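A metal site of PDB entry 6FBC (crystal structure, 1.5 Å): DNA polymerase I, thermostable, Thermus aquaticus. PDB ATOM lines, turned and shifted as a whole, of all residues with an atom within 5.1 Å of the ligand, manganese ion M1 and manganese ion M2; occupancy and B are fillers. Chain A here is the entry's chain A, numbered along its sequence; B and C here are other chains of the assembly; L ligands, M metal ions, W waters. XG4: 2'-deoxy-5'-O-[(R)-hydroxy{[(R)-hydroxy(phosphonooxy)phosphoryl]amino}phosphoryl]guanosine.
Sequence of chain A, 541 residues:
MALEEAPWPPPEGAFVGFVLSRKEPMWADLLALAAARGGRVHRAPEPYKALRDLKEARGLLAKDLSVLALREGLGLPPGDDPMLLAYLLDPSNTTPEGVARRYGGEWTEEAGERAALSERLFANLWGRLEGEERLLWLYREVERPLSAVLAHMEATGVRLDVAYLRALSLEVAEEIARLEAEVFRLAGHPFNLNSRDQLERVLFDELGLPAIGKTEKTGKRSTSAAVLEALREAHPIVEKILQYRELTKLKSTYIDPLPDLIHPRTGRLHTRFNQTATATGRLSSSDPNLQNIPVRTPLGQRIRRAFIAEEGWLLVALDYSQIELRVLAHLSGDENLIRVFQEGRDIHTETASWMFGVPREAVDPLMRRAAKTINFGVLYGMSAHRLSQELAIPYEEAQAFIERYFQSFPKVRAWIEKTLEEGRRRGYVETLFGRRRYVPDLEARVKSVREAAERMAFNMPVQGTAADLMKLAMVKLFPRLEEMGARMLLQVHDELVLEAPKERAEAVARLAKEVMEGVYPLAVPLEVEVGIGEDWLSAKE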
ATOM      1  N   ARG A 282       0.348   0.931  -0.826  1.00  0.00           N
ATOM      2  CA  ARG A 282      -0.289   1.282  -2.083  1.00  0.00           C
ATOM      3  C   ARG A 282      -0.190   0.148  -3.096  1.00  0.00           C
ATOM      4  O   ARG A 282       0.731  -0.686  -3.046  1.00  0.00           O
ATOM      5  CB  ARG A 282       0.358   2.527  -2.677  1.00  0.00           C
ATOM      6  CG  ARG A 282      -0.174   3.824  -2.133  1.00  0.00           C
ATOM      7  CD  ARG A 282       0.391   4.954  -2.942  1.00  0.00           C
ATOM      8  NE  ARG A 282      -0.269   6.215  -2.674  1.00  0.00           N
ATOM      9  CZ  ARG A 282      -0.038   7.316  -3.375  1.00  0.00           C
ATOM     10  NH1 ARG A 282       0.838   7.303  -4.370  1.00  0.00           N
ATOM     11  NH2 ARG A 282      -0.674   8.435  -3.083  1.00  0.00           N
ATOM     12  N   ASP A 319     -13.297  10.094  -6.360  1.00  0.00           N
ATOM     13  CA  ASP A 319     -11.993  10.453  -5.812  1.00  0.00           C
ATOM     14  C   ASP A 319     -12.153  11.043  -4.426  1.00  0.00           C
ATOM     15  O   ASP A 319     -12.942  11.976  -4.241  1.00  0.00           O
ATOM     16  CB  ASP A 319     -11.280  11.449  -6.750  1.00  0.00           C
ATOM     17  CG  ASP A 319      -9.899  11.789  -6.274  1.00  0.00           C
ATOM     18  OD1 ASP A 319      -9.807  12.355  -5.180  1.00  0.00           O
ATOM     19  OD2 ASP A 319      -8.937  11.442  -6.985  1.00  0.00           O
ATOM     20  N   TYR A 320     -11.416  10.504  -3.451  1.00  0.00           N
ATOM     21  CA  TYR A 320     -11.518  10.995  -2.075  1.00  0.00           C
ATOM     22  C   TYR A 320     -11.022  12.421  -1.990  1.00  0.00           C
ATOM     23  O   TYR A 320      -9.943  12.742  -2.507  1.00  0.00           O
ATOM     24  CB  TYR A 320     -10.717  10.115  -1.119  1.00  0.00           C
ATOM     25  CG  TYR A 320     -11.363   8.803  -0.687  1.00  0.00           C
ATOM     26  CD1 TYR A 320     -12.355   8.775   0.267  1.00  0.00           C
ATOM     27  CD2 TYR A 320     -10.925   7.590  -1.204  1.00  0.00           C
ATOM     28  CE1 TYR A 320     -12.939   7.577   0.671  1.00  0.00           C
ATOM     29  CE2 TYR A 320     -11.488   6.393  -0.810  1.00  0.00           C
ATOM     30  CZ  TYR A 320     -12.491   6.388   0.127  1.00  0.00           C
ATOM     31  OH  TYR A 320     -13.041   5.181   0.518  1.00  0.00           O
ATOM     32  N   SER A 321     -11.781  13.270  -1.310  1.00  0.00           N
ATOM     33  CA  SER A 321     -11.365  14.655  -1.090  1.00  0.00           C
ATOM     34  C   SER A 321     -10.240  14.744  -0.067  1.00  0.00           C
ATOM     35  O   SER A 321     -10.350  14.206   1.044  1.00  0.00           O
ATOM     36  CB  SER A 321     -12.554  15.490  -0.617  1.00  0.00           C
ATOM     37  OG  SER A 321     -12.158  16.794  -0.227  1.00  0.00           O
ATOM     38  N   GLN A 322      -9.161  15.439  -0.431  1.00  0.00           N
ATOM     39  CA  GLN A 322      -8.105  15.834   0.512  1.00  0.00           C
ATOM     40  C   GLN A 322      -7.684  14.673   1.421  1.00  0.00           C
ATOM     41  O   GLN A 322      -7.522  14.827   2.629  1.00  0.00           O
ATOM     42  CB  GLN A 322      -8.574  17.031   1.349  1.00  0.00           C
ATOM     43  CG  GLN A 322      -8.970  18.268   0.564  1.00  0.00           C
ATOM     44  CD  GLN A 322      -9.498  19.378   1.461  1.00  0.00           C
ATOM     45  OE1 GLN A 322      -8.729  20.139   2.054  1.00  0.00           O
ATOM     46  NE2 GLN A 322     -10.812  19.449   1.595  1.00  0.00           N
ATOM     47  N   ILE A 323      -7.484  13.505   0.822  1.00  0.00           N
ATOM     48  CA  ILE A 323      -7.596  12.277   1.602  1.00  0.00           C
ATOM     49  C   ILE A 323      -6.502  12.173   2.651  1.00  0.00           C
ATOM     50  O   ILE A 323      -6.775  11.821   3.806  1.00  0.00           O
ATOM     51  CB  ILE A 323      -7.631  11.036   0.685  1.00  0.00           C
ATOM     52  CG1 ILE A 323      -7.885   9.769   1.516  1.00  0.00           C
ATOM     53  CG2 ILE A 323      -6.334  10.864  -0.098  1.00  0.00           C
ATOM     54  CD1 ILE A 323      -9.168   9.796   2.325  1.00  0.00           C
ATOM     55  N   GLU A 324      -5.241  12.479   2.308  1.00  0.00           N
ATOM     56  CA  GLU A 324      -4.199  12.299   3.301  1.00  0.00           C
ATOM     57  C   GLU A 324      -4.261  13.358   4.406  1.00  0.00           C
ATOM     58  O   GLU A 324      -3.801  13.103   5.522  1.00  0.00           O
ATOM     59  CB  GLU A 324      -2.828  12.243   2.634  1.00  0.00           C
ATOM     60  CG  GLU A 324      -2.513  10.821   2.138  1.00  0.00           C
ATOM     61  CD  GLU A 324      -1.115  10.628   1.554  1.00  0.00           C
ATOM     62  OE1 GLU A 324      -0.173  11.323   1.989  1.00  0.00           O
ATOM     63  OE2 GLU A 324      -1.001   9.785   0.641  1.00  0.00           O
ATOM     64  N   LEU A 325      -4.865  14.522   4.131  1.00  0.00           N
ATOM     65  CA  LEU A 325      -5.066  15.489   5.212  1.00  0.00           C
ATOM     66  C   LEU A 325      -6.166  15.035   6.152  1.00  0.00           C
ATOM     67  O   LEU A 325      -6.095  15.285   7.366  1.00  0.00           O
ATOM     68  CB  LEU A 325      -5.372  16.875   4.646  1.00  0.00           C
ATOM     69  CG  LEU A 325      -4.226  17.531   3.883  1.00  0.00           C
ATOM     70  CD1 LEU A 325      -4.698  18.820   3.196  1.00  0.00           C
ATOM     71  CD2 LEU A 325      -3.049  17.833   4.823  1.00  0.00           C
ATOM     72  N   HIS A 348      -6.566  22.805   0.134  1.00  0.00           N
ATOM     73  CA  HIS A 348      -5.938  23.010  -1.167  1.00  0.00           C
ATOM     74  C   HIS A 348      -6.423  24.315  -1.807  1.00  0.00           C
ATOM     75  O   HIS A 348      -5.628  25.059  -2.384  1.00  0.00           O
ATOM     76  CB  HIS A 348      -6.227  21.836  -2.110  1.00  0.00           C
ATOM     77  CG  HIS A 348      -5.659  20.529  -1.649  1.00  0.00           C
ATOM     78  ND1 HIS A 348      -4.593  20.429  -0.776  1.00  0.00           N
ATOM     79  CD2 HIS A 348      -6.017  19.258  -1.946  1.00  0.00           C
ATOM     80  CE1 HIS A 348      -4.316  19.153  -0.565  1.00  0.00           C
ATOM     81  NE2 HIS A 348      -5.171  18.426  -1.256  1.00  0.00           N
ATOM     82  N   ARG A 368      -5.446  24.643  -8.067  1.00  0.00           N
ATOM     83  CA  ARG A 368      -5.688  23.854  -6.861  1.00  0.00           C
ATOM     84  C   ARG A 368      -4.770  22.631  -6.820  1.00  0.00           C
ATOM     85  O   ARG A 368      -4.230  22.293  -5.757  1.00  0.00           O
ATOM     86  CB  ARG A 368      -7.154  23.434  -6.803  1.00  0.00           C
ATOM     87  CG  ARG A 368      -7.566  22.771  -5.502  1.00  0.00           C
ATOM     88  CD  ARG A 368      -9.095  22.585  -5.392  1.00  0.00           C
ATOM     89  NE  ARG A 368      -9.415  21.797  -4.211  1.00  0.00           N
ATOM     90  CZ  ARG A 368      -9.200  20.490  -4.111  1.00  0.00           C
ATOM     91  NH1 ARG A 368      -8.686  19.814  -5.127  1.00  0.00           N
ATOM     92  NH2 ARG A 368      -9.506  19.849  -2.988  1.00  0.00           N
ATOM     93  N   LYS A 372      -2.084  21.721  -4.007  1.00  0.00           N
ATOM     94  CA  LYS A 372      -2.004  20.405  -3.391  1.00  0.00           C
ATOM     95  C   LYS A 372      -0.550  19.976  -3.217  1.00  0.00           C
ATOM     96  O   LYS A 372      -0.154  19.480  -2.158  1.00  0.00           O
ATOM     97  CB  LYS A 372      -2.783  19.389  -4.217  1.00  0.00           C
ATOM     98  CG  LYS A 372      -2.621  17.931  -3.771  1.00  0.00           C
ATOM     99  CD  LYS A 372      -2.319  16.989  -4.950  1.00  0.00           C
ATOM    100  CE  LYS A 372      -0.907  17.161  -5.494  1.00  0.00           C
ATOM    101  NZ  LYS A 372      -0.610  16.119  -6.536  1.00  0.00           N
ATOM    102  N   THR A 373       0.279  20.191  -4.249  1.00  0.00           N
ATOM    103  CA  THR A 373       1.680  19.825  -4.174  1.00  0.00           C
ATOM    104  C   THR A 373       2.373  20.569  -3.038  1.00  0.00           C
ATOM    105  O   THR A 373       3.188  19.995  -2.318  1.00  0.00           O
ATOM    106  CB  THR A 373       2.375  20.129  -5.505  1.00  0.00           C
ATOM    107  OG1 THR A 373       1.639  19.514  -6.564  1.00  0.00           O
ATOM    108  CG2 THR A 373       3.801  19.621  -5.513  1.00  0.00           C
ATOM    109  N   PHE A 376       1.225  19.143   0.592  1.00  0.00           N
ATOM    110  CA  PHE A 376       1.863  17.887   0.971  1.00  0.00           C
ATOM    111  C   PHE A 376       3.381  18.019   0.991  1.00  0.00           C
ATOM    112  O   PHE A 376       4.044  17.424   1.845  1.00  0.00           O
ATOM    113  CB  PHE A 376       1.402  16.772   0.034  1.00  0.00           C
ATOM    114  CG  PHE A 376      -0.039  16.427   0.215  1.00  0.00           C
ATOM    115  CD1 PHE A 376      -0.507  16.015   1.462  1.00  0.00           C
ATOM    116  CD2 PHE A 376      -0.945  16.548  -0.814  1.00  0.00           C
ATOM    117  CE1 PHE A 376      -1.837  15.716   1.656  1.00  0.00           C
ATOM    118  CE2 PHE A 376      -2.294  16.247  -0.610  1.00  0.00           C
ATOM    119  CZ  PHE A 376      -2.732  15.836   0.618  1.00  0.00           C
ATOM    120  N   GLY A 377       3.942  18.829   0.089  1.00  0.00           N
ATOM    121  CA  GLY A 377       5.374  19.083   0.148  1.00  0.00           C
ATOM    122  C   GLY A 377       5.785  19.603   1.506  1.00  0.00           C
ATOM    123  O   GLY A 377       6.698  19.090   2.142  1.00  0.00           O
ATOM    124  N   TYR A 380       5.342  16.911   4.492  1.00  0.00           N
ATOM    125  CA  TYR A 380       6.308  15.822   4.561  1.00  0.00           C
ATOM    126  C   TYR A 380       7.763  16.300   4.499  1.00  0.00           C
ATOM    127  O   TYR A 380       8.654  15.483   4.267  1.00  0.00           O
ATOM    128  CB  TYR A 380       6.009  14.809   3.450  1.00  0.00           C
ATOM    129  CG  TYR A 380       4.643  14.148   3.623  1.00  0.00           C
ATOM    130  CD1 TYR A 380       4.349  13.428   4.775  1.00  0.00           C
ATOM    131  CD2 TYR A 380       3.680  14.233   2.632  1.00  0.00           C
ATOM    132  CE1 TYR A 380       3.111  12.828   4.953  1.00  0.00           C
ATOM    133  CE2 TYR A 380       2.426  13.615   2.795  1.00  0.00           C
ATOM    134  CZ  TYR A 380       2.157  12.917   3.962  1.00  0.00           C
ATOM    135  OH  TYR A 380       0.940  12.295   4.170  1.00  0.00           O
ATOM    136  N   ASN A 459       5.806   9.592   6.690  1.00  0.00           N
ATOM    137  CA  ASN A 459       4.867   9.582   5.573  1.00  0.00           C
ATOM    138  C   ASN A 459       4.056   8.292   5.540  1.00  0.00           C
ATOM    139  O   ASN A 459       2.867   8.298   5.206  1.00  0.00           O
ATOM    140  CB  ASN A 459       5.615   9.780   4.261  1.00  0.00           C
ATOM    141  CG  ASN A 459       4.745   9.540   3.040  1.00  0.00           C
ATOM    142  OD1 ASN A 459       4.683   8.425   2.508  1.00  0.00           O
ATOM    143  ND2 ASN A 459       4.063  10.584   2.577  1.00  0.00           N
ATOM    144  N   VAL A 492      -6.705   4.571  -8.901  1.00  0.00           N
ATOM    145  CA  VAL A 492      -5.571   5.500  -8.963  1.00  0.00           C
ATOM    146  C   VAL A 492      -5.335   6.063  -7.566  1.00  0.00           C
ATOM    147  O   VAL A 492      -5.446   7.260  -7.322  1.00  0.00           O
ATOM    148  CB  VAL A 492      -5.797   6.628 -10.000  1.00  0.00           C
ATOM    149  CG1 VAL A 492      -4.484   7.312 -10.306  1.00  0.00           C
ATOM    150  CG2 VAL A 492      -6.384   6.077 -11.294  1.00  0.00           C
ATOM    151  N   ASP A 494      -6.457   6.926  -4.656  1.00  0.00           N
ATOM    152  CA  ASP A 494      -7.629   7.330  -3.884  1.00  0.00           C
ATOM    153  C   ASP A 494      -8.817   7.541  -4.802  1.00  0.00           C
ATOM    154  O   ASP A 494      -9.749   8.266  -4.455  1.00  0.00           O
ATOM    155  CB  ASP A 494      -7.356   8.601  -3.069  1.00  0.00           C
ATOM    156  CG  ASP A 494      -7.414   9.865  -3.913  1.00  0.00           C
ATOM    157  OD1 ASP A 494      -7.100   9.785  -5.127  1.00  0.00           O
ATOM    158  OD2 ASP A 494      -7.764  10.937  -3.372  1.00  0.00           O
ATOM    159  N   GLU A 495      -8.799   6.898  -5.959  1.00  0.00           N
ATOM    160  CA  GLU A 495      -9.788   7.098  -6.993  1.00  0.00           C
ATOM    161  C   GLU A 495     -10.142   5.746  -7.599  1.00  0.00           C
ATOM    162  O   GLU A 495      -9.265   4.874  -7.737  1.00  0.00           O
ATOM    163  CB  GLU A 495      -9.263   8.072  -8.081  1.00  0.00           C
ATOM    164  CG  GLU A 495     -10.088   8.152  -9.360  1.00  0.00           C
ATOM    165  CD  GLU A 495      -9.403   8.961 -10.445  1.00  0.00           C
ATOM    166  OE1 GLU A 495      -8.301   9.503 -10.209  1.00  0.00           O
ATOM    167  OE2 GLU A 495      -9.987   9.039 -11.549  1.00  0.00           O
ATOM    168  N   LYS A 540     -14.363  13.315 -14.410  1.00  0.00           N
ATOM    169  CA  LYS A 540     -13.761  13.942 -13.236  1.00  0.00           C
ATOM    170  C   LYS A 540     -14.095  15.438 -13.130  1.00  0.00           C
ATOM    171  O   LYS A 540     -13.468  16.138 -12.339  1.00  0.00           O
ATOM    172  CB  LYS A 540     -12.248  13.745 -13.230  1.00  0.00           C
ATOM    173  CG  LYS A 540     -11.817  12.312 -12.913  1.00  0.00           C
ATOM    174  CD  LYS A 540     -10.483  12.238 -12.183  1.00  0.00           C
ATOM    175  CE  LYS A 540     -10.637  12.606 -10.710  1.00  0.00           C
ATOM    176  NZ  LYS A 540      -9.324  12.587  -9.983  1.00  0.00           N
ATOM    177  O   D4B B  12      -1.675   9.955  -8.232  1.00  0.00           O
ATOM    178  C1' D4B B  12      -1.185   9.941  -6.932  1.00  0.00           C
ATOM    179  C10 D4B B  12      -0.381  16.374 -11.190  1.00  0.00           C
ATOM    180  C11 D4B B  12      -0.714  17.571 -11.781  1.00  0.00           C
ATOM    181  C12 D4B B  12       0.963  17.579  -9.549  1.00  0.00           C
ATOM    182  C13 D4B B  12       0.610  18.771 -10.152  1.00  0.00           C
ATOM    183  C14 D4B B  12      -0.250  18.785 -11.248  1.00  0.00           C
ATOM    184  C15 D4B B  12      -0.746  19.961 -11.841  1.00  0.00           C
ATOM    185  C16 D4B B  12      -1.093  21.017 -12.220  1.00  0.00           C
ATOM    186  C2  D4B B  12       0.901  10.949  -6.041  1.00  0.00           C
ATOM    187  C2' D4B B  12      -2.336  10.339  -5.947  1.00  0.00           C
ATOM    188  C3' D4B B  12      -3.468  10.741  -6.872  1.00  0.00           C
ATOM    189  C4  D4B B  12      -0.253  12.127  -7.797  1.00  0.00           C
ATOM    190  C4' D4B B  12      -3.089   9.943  -8.133  1.00  0.00           C
ATOM    191  C5  D4B B  12       0.811  13.062  -7.898  1.00  0.00           C
ATOM    192  C5' D4B B  12      -3.697  10.709  -9.344  1.00  0.00           C
ATOM    193  C6  D4B B  12       1.899  12.818  -7.037  1.00  0.00           C
ATOM    194  C7  D4B B  12       0.726  14.179  -8.711  1.00  0.00           C
ATOM    195  C8  D4B B  12       0.608  15.166  -9.358  1.00  0.00           C
ATOM    196  C9  D4B B  12       0.444  16.376 -10.051  1.00  0.00           C
ATOM    197  N1  D4B B  12       1.949  11.840  -6.140  1.00  0.00           N
ATOM    198  N3  D4B B  12      -0.187  11.074  -6.921  1.00  0.00           N
ATOM    199  N6  D4B B  12       3.044  13.597  -7.131  1.00  0.00           N
ATOM    200  O1  D4B B  12      -3.160  11.966  -9.407  1.00  0.00           O
ATOM    201  O2  D4B B  12       0.888  10.071  -5.185  1.00  0.00           O
ATOM    202  OP1 D4B B  12      -4.911  12.647 -11.068  1.00  0.00           O
ATOM    203  O3' D4B B  12      -4.721  10.362  -6.382  1.00  0.00           O
ATOM    204  P   D4B B  12      -3.387  12.827 -10.897  1.00  0.00           P
ATOM    205  OP2 D4B B  12      -2.944  14.229 -10.526  1.00  0.00           O
ATOM    206  P    DC C   4      13.310  19.040  -0.344  1.00  0.00           P
ATOM    207  OP1  DC C   4      13.385  18.856  -1.807  1.00  0.00           O
ATOM    208  OP2  DC C   4      13.350  20.391   0.235  1.00  0.00           O
ATOM    209  O5'  DC C   4      11.945  18.388   0.126  1.00  0.00           O
ATOM    210  C5'  DC C   4      11.680  17.063  -0.193  1.00  0.00           C
ATOM    211  C4'  DC C   4      10.558  16.534   0.659  1.00  0.00           C
ATOM    212  O4'  DC C   4       9.363  17.310   0.408  1.00  0.00           O
ATOM    213  C3'  DC C   4      10.166  15.102   0.379  1.00  0.00           C
ATOM    214  O3'  DC C   4      10.995  14.207   1.083  1.00  0.00           O
ATOM    215  C2'  DC C   4       8.714  15.072   0.835  1.00  0.00           C
ATOM    216  C1'  DC C   4       8.230  16.452   0.423  1.00  0.00           C
ATOM    217  N1   DC C   4       7.566  16.519  -0.916  1.00  0.00           N
ATOM    218  C2   DC C   4       6.327  15.905  -1.080  1.00  0.00           C
ATOM    219  O2   DC C   4       5.845  15.291  -0.137  1.00  0.00           O
ATOM    220  N3   DC C   4       5.709  15.996  -2.271  1.00  0.00           N
ATOM    221  C4   DC C   4       6.261  16.663  -3.273  1.00  0.00           C
ATOM    222  N4   DC C   4       5.587  16.712  -4.433  1.00  0.00           N
ATOM    223  C5   DC C   4       7.528  17.314  -3.129  1.00  0.00           C
ATOM    224  C6   DC C   4       8.137  17.220  -1.938  1.00  0.00           C
ATOM    225  P    DG C   5      11.606  12.937   0.329  1.00  0.00           P
ATOM    226  OP1  DG C   5      12.701  12.420   1.191  1.00  0.00           O
ATOM    227  OP2  DG C   5      11.876  13.296  -1.085  1.00  0.00           O
ATOM    228  O5'  DG C   5      10.360  11.917   0.299  1.00  0.00           O
ATOM    229  C5'  DG C   5       9.921  11.339   1.516  1.00  0.00           C
ATOM    230  C4'  DG C   5       8.575  10.693   1.355  1.00  0.00           C
ATOM    231  O4'  DG C   5       7.632  11.688   0.893  1.00  0.00           O
ATOM    232  C3'  DG C   5       8.491   9.581   0.321  1.00  0.00           C
ATOM    233  O3'  DG C   5       8.951   8.320   0.855  1.00  0.00           O
ATOM    234  C2'  DG C   5       7.005   9.578  -0.009  1.00  0.00           C
ATOM    235  C1'  DG C   5       6.661  11.068   0.076  1.00  0.00           C
ATOM    236  N9   DG C   5       6.629  11.743  -1.210  1.00  0.00           N
ATOM    237  C8   DG C   5       7.525  12.663  -1.716  1.00  0.00           C
ATOM    238  N7   DG C   5       7.221  13.083  -2.916  1.00  0.00           N
ATOM    239  C5   DG C   5       6.025  12.411  -3.203  1.00  0.00           C
ATOM    240  C6   DG C   5       5.206  12.479  -4.339  1.00  0.00           C
ATOM    241  O6   DG C   5       5.364  13.162  -5.369  1.00  0.00           O
ATOM    242  N1   DG C   5       4.092  11.623  -4.226  1.00  0.00           N
ATOM    243  C2   DG C   5       3.829  10.835  -3.132  1.00  0.00           C
ATOM    244  N2   DG C   5       2.731  10.067  -3.195  1.00  0.00           N
ATOM    245  N3   DG C   5       4.587  10.773  -2.058  1.00  0.00           N
ATOM    246  C4   DG C   5       5.673  11.588  -2.174  1.00  0.00           C
HETATM  247  N1  XG4 L   1       3.224  14.682  -2.530  1.00  0.00           N
HETATM  248  C2  XG4 L   1       2.875  13.747  -1.584  1.00  0.00           C
HETATM  249  N2  XG4 L   1       3.714  13.573  -0.568  1.00  0.00           N
HETATM  250  N3  XG4 L   1       1.744  13.041  -1.633  1.00  0.00           N
HETATM  251  C4  XG4 L   1       0.989  13.354  -2.690  1.00  0.00           C
HETATM  252  C5  XG4 L   1       1.248  14.260  -3.693  1.00  0.00           C
HETATM  253  C6  XG4 L   1       2.468  15.017  -3.627  1.00  0.00           C
HETATM  254  O6  XG4 L   1       2.829  15.898  -4.403  1.00  0.00           O
HETATM  255  N7  XG4 L   1       0.190  14.301  -4.597  1.00  0.00           N
HETATM  256  C8  XG4 L   1      -0.679  13.448  -4.106  1.00  0.00           C
HETATM  257  N9  XG4 L   1      -0.271  12.858  -2.948  1.00  0.00           N
HETATM  258  PA  XG4 L   1      -5.079  13.640  -5.037  1.00  0.00           P
HETATM  259  PB  XG4 L   1      -6.221  15.079  -2.693  1.00  0.00           P
HETATM  260  PG  XG4 L   1      -8.511  16.320  -3.893  1.00  0.00           P
HETATM  261  C1' XG4 L   1      -1.036  11.994  -2.033  1.00  0.00           C
HETATM  262  O1A XG4 L   1      -6.455  12.846  -5.201  1.00  0.00           O
HETATM  263  O1B XG4 L   1      -6.862  13.834  -2.280  1.00  0.00           O
HETATM  264  O1G XG4 L   1      -9.569  16.958  -3.014  1.00  0.00           O
HETATM  265  C2' XG4 L   1      -1.733  12.803  -0.941  1.00  0.00           C
HETATM  266  O2A XG4 L   1      -4.572  14.081  -6.320  1.00  0.00           O
HETATM  267  O2B XG4 L   1      -5.309  15.565  -1.519  1.00  0.00           O
HETATM  268  O2G XG4 L   1      -8.135  17.181  -5.100  1.00  0.00           O
HETATM  269  C3' XG4 L   1      -3.120  13.015  -1.541  1.00  0.00           C
HETATM  270  O3' XG4 L   1      -4.084  13.241  -0.508  1.00  0.00           O
HETATM  271  N3A XG4 L   1      -5.319  14.913  -4.054  1.00  0.00           N
HETATM  272  O3B XG4 L   1      -7.180  16.261  -3.016  1.00  0.00           O
HETATM  273  O3G XG4 L   1      -8.760  14.826  -4.291  1.00  0.00           O
HETATM  274  C4' XG4 L   1      -3.335  11.677  -2.230  1.00  0.00           C
HETATM  275  O4' XG4 L   1      -2.051  11.337  -2.784  1.00  0.00           O
HETATM  276  C5' XG4 L   1      -4.376  11.662  -3.312  1.00  0.00           C
HETATM  277  O5' XG4 L   1      -4.105  12.685  -4.269  1.00  0.00           O
HETATM  278 MN    MN M   1      -8.267  12.865  -3.833  1.00  0.00          MN
HETATM  279 MN    MN M   2      -6.861  11.212  -6.682  1.00  0.00          MN
HETATM  280  O   HOH W   1      -2.751   8.610  -0.966  1.00  0.00           O
HETATM  281  O   HOH W   2      -2.634  15.027  -8.099  1.00  0.00           O
HETATM  282  O   HOH W   3     -11.702  14.553  -4.902  1.00  0.00           O
HETATM  283  O   HOH W   4       2.068  16.961  -6.731  1.00  0.00           O
HETATM  284  O   HOH W   5      -6.152  12.870  -8.240  1.00  0.00           O
HETATM  285  O   HOH W   6     -12.011  17.251  -3.928  1.00  0.00           O
HETATM  286  O   HOH W   7      -6.875   9.894  -8.452  1.00  0.00           O
HETATM  287  O   HOH W   8       2.030  10.636   0.462  1.00  0.00           O
HETATM  288  O   HOH W   9      -8.236  14.829  -7.097  1.00  0.00           O
HETATM  289  O   HOH W  10      -5.474  17.438  -5.723  1.00  0.00           O
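O2G of the ligand lies within salt-bridge range of NH1 of Arg 368 (2.7 Å).
N2 of the ligand is in hydrogen-bond range of O2 of DC 4 of chain C (2.8 Å).
NZ of Lys 372 sits at hydrogen-bond distance from N7 of the ligand (2.8 Å).
An oxygen (O2B) of the ligand sits at hydrogen-bond distance from a ring nitrogen (NE2) of His 348.
An oxygen (O1G) of the ligand sits at hydrogen-bond distance from the backbone NH of Gln 322 (3.0 Å).
An oxygen (O3') of the ligand lies within hydrogen-bond range of the backbone NH (N) of Glu 324 (3.1 Å).
The backbone NH of Ile 323 lies close to an oxygen (O1B) of the ligand (3.2 Å).
N3 of DG 5 of chain C sits close to a nitrogen (N2) of the ligand, at 3.3 Å.
The guanidinium group of Arg 282 is in hydrogen-bond range of an oxygen (O4') of the ligand (3.2 Å).
The nearest printed residue that does not touch manganese ion M2 is Glu 495 (4.2 Å).
Of the 23 residues printed, 3 come within 4 Å of manganese ion M1.
OD2 of Asp 494 binds manganese ion M1 (2.0 Å).
O3G of the ligand binds manganese ion M1.
OD1 of Asp 319 is bound to manganese ion M1, at 2.1 Å.
O of Tyr 320 binds manganese ion M1, 2.1 Å away.
O1A of the ligand is bound to manganese ion M1, at 2.3 Å.
O1B of the ligand is bound to manganese ion M1, at 2.3 Å.
Water W5 lies within hydrogen-bond range of O2A of the ligand and OP1 of D4B 12 of chain B.
Water W4 lies within hydrogen-bond range of OG1 of Thr 373, O6 of the ligand and NZ of Lys 372.
Water W2 lies within hydrogen-bond range of OP2 of D4B 12 of chain B (2.6 Å), NZ of Lys 372 (2.8 Å) and O2A of the ligand (2.8 Å).
Water W8 lies within hydrogen-bond range of OE1 of Glu 324 (2.8 Å), ND2 of Asn 459 (2.9 Å) and N3 of the ligand (3.2 Å).
Water W1 lies within hydrogen-bond range of OE2 of Glu 324 (2.7 Å), NH2 of Arg 282 (3.0 Å) and O4' of the ligand (3.4 Å).
CA of Ser 321 touches O1G of the ligand (3.5 Å).
Phe 376 touches the ligand (CZ to O3', 3.1 Å).
Tyr 380 touches the ligand.
Of the 23 residues printed, 16 come within 4 Å of the ligand.
The nearest printed residue that does not touch the ligand is Thr 373 (4.005 Å).
The side-chain carboxylate of Asp 319 sits close to the side-chain amino group of Lys 540, 3.2 Å away.
N2 of DG 5 of chain C lies close to O2 of D4B 12 of chain B (2.7 Å).
The guanidinium group of Arg 282 is in hydrogen-bond range of O2 of D4B 12 of chain B, at 2.9 Å.
The side-chain amide nitrogen (NE2) of Gln 322 is in hydrogen-bond range of the side-chain hydroxyl (OG) of Ser 321 (3.5 Å).
The side-chain carboxylate (OE2) of Glu 324 is in salt-bridge range of the guanidinium group (NH2) of Arg 282 (3.97 Å).
OH of Tyr 380 is in hydrogen-bond range of OE1 of Glu 324 (2.6 Å).
Manganese ion M2 is bound by OD2 of Asp 319 (2.1 Å), OD1 of Asp 494 (2.1 Å), water W7 (2.2 Å), O1A of the ligand (2.2 Å), O3' of D4B 12 of chain B (2.3 Å) and water W5 (2.4 Å).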
